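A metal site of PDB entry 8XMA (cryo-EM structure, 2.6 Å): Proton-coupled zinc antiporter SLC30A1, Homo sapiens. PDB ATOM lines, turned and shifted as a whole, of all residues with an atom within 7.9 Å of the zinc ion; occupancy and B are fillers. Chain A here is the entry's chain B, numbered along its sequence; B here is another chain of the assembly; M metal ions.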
ATOM      1  N   LYS A 404      18.908 -31.426  -8.598  1.00  0.00           N
ATOM      2  CA  LYS A 404      19.242 -30.084  -8.134  1.00  0.00           C
ATOM      3  C   LYS A 404      18.267 -29.053  -8.669  1.00  0.00           C
ATOM      4  O   LYS A 404      17.833 -28.162  -7.946  1.00  0.00           O
ATOM      5  CB  LYS A 404      20.674 -29.726  -8.534  1.00  0.00           C
ATOM      6  CG  LYS A 404      21.123 -28.349  -8.059  1.00  0.00           C
ATOM      7  CD  LYS A 404      21.172 -28.245  -6.544  1.00  0.00           C
ATOM      8  CE  LYS A 404      22.307 -29.081  -5.977  1.00  0.00           C
ATOM      9  NZ  LYS A 404      22.418 -28.938  -4.501  1.00  0.00           N
ATOM     10  N   ASP A 405      17.892 -29.174  -9.946  1.00  0.00           N
ATOM     11  CA  ASP A 405      16.912 -28.258 -10.527  1.00  0.00           C
ATOM     12  C   ASP A 405      15.546 -28.412  -9.857  1.00  0.00           C
ATOM     13  O   ASP A 405      14.859 -27.419  -9.597  1.00  0.00           O
ATOM     14  CB  ASP A 405      16.798 -28.493 -12.026  1.00  0.00           C
ATOM     15  CG  ASP A 405      18.046 -28.073 -12.781  1.00  0.00           C
ATOM     16  OD1 ASP A 405      18.738 -27.140 -12.316  1.00  0.00           O
ATOM     17  OD2 ASP A 405      18.331 -28.666 -13.845  1.00  0.00           O
ATOM     18  N   PHE A 407      14.933 -29.387  -6.799  1.00  0.00           N
ATOM     19  CA  PHE A 407      15.019 -28.737  -5.498  1.00  0.00           C
ATOM     20  C   PHE A 407      15.073 -27.215  -5.647  1.00  0.00           C
ATOM     21  O   PHE A 407      14.529 -26.490  -4.798  1.00  0.00           O
ATOM     22  CB  PHE A 407      16.258 -29.245  -4.752  1.00  0.00           C
ATOM     23  CG  PHE A 407      15.985 -30.456  -3.907  1.00  0.00           C
ATOM     24  CD1 PHE A 407      15.069 -30.403  -2.874  1.00  0.00           C
ATOM     25  CD2 PHE A 407      16.656 -31.641  -4.142  1.00  0.00           C
ATOM     26  CE1 PHE A 407      14.823 -31.513  -2.098  1.00  0.00           C
ATOM     27  CE2 PHE A 407      16.412 -32.756  -3.375  1.00  0.00           C
ATOM     28  CZ  PHE A 407      15.495 -32.694  -2.346  1.00  0.00           C
ATOM     29  N   HIS A 408      15.708 -26.722  -6.710  1.00  0.00           N
ATOM     30  CA  HIS A 408      15.863 -25.290  -6.891  1.00  0.00           C
ATOM     31  C   HIS A 408      14.551 -24.621  -7.302  1.00  0.00           C
ATOM     32  O   HIS A 408      14.372 -23.428  -7.063  1.00  0.00           O
ATOM     33  CB  HIS A 408      16.958 -25.020  -7.931  1.00  0.00           C
ATOM     34  CG  HIS A 408      17.114 -23.584  -8.298  1.00  0.00           C
ATOM     35  ND1 HIS A 408      17.930 -22.717  -7.606  1.00  0.00           N
ATOM     36  CD2 HIS A 408      16.563 -22.854  -9.298  1.00  0.00           C
ATOM     37  CE1 HIS A 408      17.875 -21.512  -8.149  1.00  0.00           C
ATOM     38  NE2 HIS A 408      17.048 -21.573  -9.179  1.00  0.00           N
ATOM     39  N   ASN A 409      13.645 -25.377  -7.924  1.00  0.00           N
ATOM     40  CA  ASN A 409      12.334 -24.826  -8.238  1.00  0.00           C
ATOM     41  C   ASN A 409      11.608 -24.399  -6.969  1.00  0.00           C
ATOM     42  O   ASN A 409      10.969 -23.337  -6.928  1.00  0.00           O
ATOM     43  CB  ASN A 409      11.504 -25.843  -9.018  1.00  0.00           C
ATOM     44  CG  ASN A 409      12.174 -26.274 -10.310  1.00  0.00           C
ATOM     45  OD1 ASN A 409      12.904 -25.496 -10.931  1.00  0.00           O
ATOM     46  ND2 ASN A 409      11.936 -27.501 -10.717  1.00  0.00           N
ATOM     47  N   HIS A 410      11.671 -25.221  -5.918  1.00  0.00           N
ATOM     48  CA  HIS A 410      11.226 -24.810  -4.605  1.00  0.00           C
ATOM     49  C   HIS A 410      12.329 -24.005  -3.912  1.00  0.00           C
ATOM     50  O   HIS A 410      13.444 -23.886  -4.408  1.00  0.00           O
ATOM     51  CB  HIS A 410      10.822 -26.023  -3.770  1.00  0.00           C
ATOM     52  CG  HIS A 410       9.932 -26.979  -4.492  1.00  0.00           C
ATOM     53  ND1 HIS A 410      10.404 -27.831  -5.467  1.00  0.00           N
ATOM     54  CD2 HIS A 410       8.606 -27.226  -4.387  1.00  0.00           C
ATOM     55  CE1 HIS A 410       9.404 -28.565  -5.929  1.00  0.00           C
ATOM     56  NE2 HIS A 410       8.297 -28.212  -5.294  1.00  0.00           N
ATOM     57  N   GLY A 411      11.992 -23.462  -2.744  1.00  0.00           N
ATOM     58  CA  GLY A 411      12.942 -22.628  -2.024  1.00  0.00           C
ATOM     59  C   GLY A 411      14.045 -23.405  -1.322  1.00  0.00           C
ATOM     60  O   GLY A 411      14.328 -23.165  -0.153  1.00  0.00           O
ATOM     61  N   ILE A 412      14.677 -24.326  -2.037  1.00  0.00           N
ATOM     62  CA  ILE A 412      15.743 -25.163  -1.487  1.00  0.00           C
ATOM     63  C   ILE A 412      16.961 -25.042  -2.396  1.00  0.00           C
ATOM     64  O   ILE A 412      16.859 -25.288  -3.597  1.00  0.00           O
ATOM     65  CB  ILE A 412      15.317 -26.631  -1.367  1.00  0.00           C
ATOM     66  CG1 ILE A 412      14.265 -26.785  -0.261  1.00  0.00           C
ATOM     67  CG2 ILE A 412      16.509 -27.512  -1.086  1.00  0.00           C
ATOM     68  CD1 ILE A 412      13.537 -28.108  -0.304  1.00  0.00           C
ATOM     69  N   HIS A 413      18.095 -24.665  -1.809  1.00  0.00           N
ATOM     70  CA  HIS A 413      19.335 -24.514  -2.578  1.00  0.00           C
ATOM     71  C   HIS A 413      20.538 -25.197  -1.946  1.00  0.00           C
ATOM     72  O   HIS A 413      21.554 -25.347  -2.639  1.00  0.00           O
ATOM     73  CB  HIS A 413      19.660 -23.026  -2.779  1.00  0.00           C
ATOM     74  CG  HIS A 413      18.526 -22.246  -3.364  1.00  0.00           C
ATOM     75  ND1 HIS A 413      18.289 -22.164  -4.722  1.00  0.00           N
ATOM     76  CD2 HIS A 413      17.561 -21.499  -2.769  1.00  0.00           C
ATOM     77  CE1 HIS A 413      17.229 -21.411  -4.939  1.00  0.00           C
ATOM     78  NE2 HIS A 413      16.768 -20.998  -3.769  1.00  0.00           N
ATOM     79  N   ALA A 414      20.464 -25.612  -0.690  1.00  0.00           N
ATOM     80  CA  ALA A 414      21.543 -26.330  -0.024  1.00  0.00           C
ATOM     81  C   ALA A 414      21.103 -27.791   0.111  1.00  0.00           C
ATOM     82  O   ALA A 414      20.360 -28.142   1.027  1.00  0.00           O
ATOM     83  CB  ALA A 414      21.871 -25.716   1.333  1.00  0.00           C
ATOM     84  N   THR A 415      21.573 -28.633  -0.801  1.00  0.00           N
ATOM     85  CA  THR A 415      21.156 -30.024  -0.857  1.00  0.00           C
ATOM     86  C   THR A 415      22.360 -30.945  -0.736  1.00  0.00           C
ATOM     87  O   THR A 415      23.506 -30.546  -0.942  1.00  0.00           O
ATOM     88  CB  THR A 415      20.393 -30.347  -2.151  1.00  0.00           C
ATOM     89  OG1 THR A 415      21.338 -30.559  -3.210  1.00  0.00           O
ATOM     90  CG2 THR A 415      19.475 -29.194  -2.527  1.00  0.00           C
ATOM     91  N   ALA B 436      25.864 -26.959  -7.963  1.00  0.00           N
ATOM     92  CA  ALA B 436      25.585 -25.716  -7.256  1.00  0.00           C
ATOM     93  C   ALA B 436      24.413 -25.002  -7.920  1.00  0.00           C
ATOM     94  O   ALA B 436      24.153 -25.172  -9.108  1.00  0.00           O
ATOM     95  CB  ALA B 436      26.808 -24.797  -7.238  1.00  0.00           C
ATOM     96  N   CYS B 437      23.704 -24.212  -7.122  1.00  0.00           N
ATOM     97  CA  CYS B 437      22.553 -23.472  -7.632  1.00  0.00           C
ATOM     98  C   CYS B 437      22.997 -22.408  -8.623  1.00  0.00           C
ATOM     99  O   CYS B 437      24.060 -21.802  -8.472  1.00  0.00           O
ATOM    100  CB  CYS B 437      21.792 -22.823  -6.475  1.00  0.00           C
ATOM    101  SG  CYS B 437      20.445 -21.732  -6.985  1.00  0.00           S
ATOM    102  N   ARG B 438      22.182 -22.201  -9.661  1.00  0.00           N
ATOM    103  CA  ARG B 438      22.530 -21.215 -10.682  1.00  0.00           C
ATOM    104  C   ARG B 438      22.568 -19.808 -10.106  1.00  0.00           C
ATOM    105  O   ARG B 438      23.488 -19.038 -10.399  1.00  0.00           O
ATOM    106  CB  ARG B 438      21.535 -21.300 -11.845  1.00  0.00           C
ATOM    107  CG  ARG B 438      21.159 -22.718 -12.235  1.00  0.00           C
ATOM    108  CD  ARG B 438      20.110 -22.719 -13.340  1.00  0.00           C
ATOM    109  NE  ARG B 438      18.956 -21.900 -13.015  1.00  0.00           N
ATOM    110  CZ  ARG B 438      17.768 -22.008 -13.582  1.00  0.00           C
ATOM    111  NH1 ARG B 438      17.535 -22.925 -14.516  1.00  0.00           N
ATOM    112  NH2 ARG B 438      16.781 -21.199 -13.210  1.00  0.00           N
ATOM    113  N   THR B 439      21.590 -19.458  -9.276  1.00  0.00           N
ATOM    114  CA  THR B 439      21.529 -18.141  -8.645  1.00  0.00           C
ATOM    115  C   THR B 439      22.072 -18.276  -7.228  1.00  0.00           C
ATOM    116  O   THR B 439      21.331 -18.317  -6.241  1.00  0.00           O
ATOM    117  CB  THR B 439      20.104 -17.593  -8.653  1.00  0.00           C
ATOM    118  OG1 THR B 439      19.293 -18.356  -7.760  1.00  0.00           O
ATOM    119  CG2 THR B 439      19.520 -17.671 -10.062  1.00  0.00           C
ATOM    120  N   GLN B 440      23.398 -18.348  -7.122  1.00  0.00           N
ATOM    121  CA  GLN B 440      24.042 -18.472  -5.824  1.00  0.00           C
ATOM    122  C   GLN B 440      23.811 -17.209  -5.000  1.00  0.00           C
ATOM    123  O   GLN B 440      23.916 -16.089  -5.505  1.00  0.00           O
ATOM    124  CB  GLN B 440      25.544 -18.721  -5.986  1.00  0.00           C
ATOM    125  CG  GLN B 440      25.900 -20.146  -6.384  1.00  0.00           C
ATOM    126  CD  GLN B 440      27.397 -20.349  -6.502  1.00  0.00           C
ATOM    127  OE1 GLN B 440      28.186 -19.412  -6.360  1.00  0.00           O
ATOM    128  NE2 GLN B 440      27.802 -21.591  -6.751  1.00  0.00           N
ATOM    129  N   CYS B 441      23.495 -17.401  -3.724  1.00  0.00           N
ATOM    130  CA  CYS B 441      23.281 -16.300  -2.800  1.00  0.00           C
ATOM    131  C   CYS B 441      23.800 -16.698  -1.427  1.00  0.00           C
ATOM    132  O   CYS B 441      23.595 -17.835  -0.984  1.00  0.00           O
ATOM    133  CB  CYS B 441      21.802 -15.910  -2.717  1.00  0.00           C
ATOM    134  SG  CYS B 441      21.426 -14.686  -1.436  1.00  0.00           S
ATOM    135  N   LYS B 444      20.994 -17.696   0.929  1.00  0.00           N
ATOM    136  CA  LYS B 444      20.199 -18.854   0.542  1.00  0.00           C
ATOM    137  C   LYS B 444      21.059 -20.115   0.464  1.00  0.00           C
ATOM    138  O   LYS B 444      20.908 -20.924  -0.448  1.00  0.00           O
ATOM    139  CB  LYS B 444      19.479 -18.610  -0.779  1.00  0.00           C
ATOM    140  CG  LYS B 444      18.181 -17.835  -0.652  1.00  0.00           C
ATOM    141  CD  LYS B 444      17.690 -17.361  -2.012  1.00  0.00           C
ATOM    142  CE  LYS B 444      17.105 -15.956  -1.927  1.00  0.00           C
ATOM    143  NZ  LYS B 444      15.786 -15.954  -1.246  1.00  0.00           N
HETATM  144 ZN    ZN M   1      19.115 -23.394  -6.105  1.00  0.00          ZN
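A ring nitrogen (ND1) of His 413 is bound to the zinc ion.
ND1 of His 408 binds the zinc ion (2.0 Å).
SG of Cys 437 of chain B is bound to the zinc ion.
SG of Cys 437 of chain B sits close to N of Thr 439 of chain B (3.4 Å).
O of Ile 412 touches the zinc ion (3.9 Å).
Of the 18 residues printed, 4 come within 4 Å of the zinc ion.
The nearest printed residue that does not touch the zinc ion is Arg 438 of chain B (4.8 Å).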
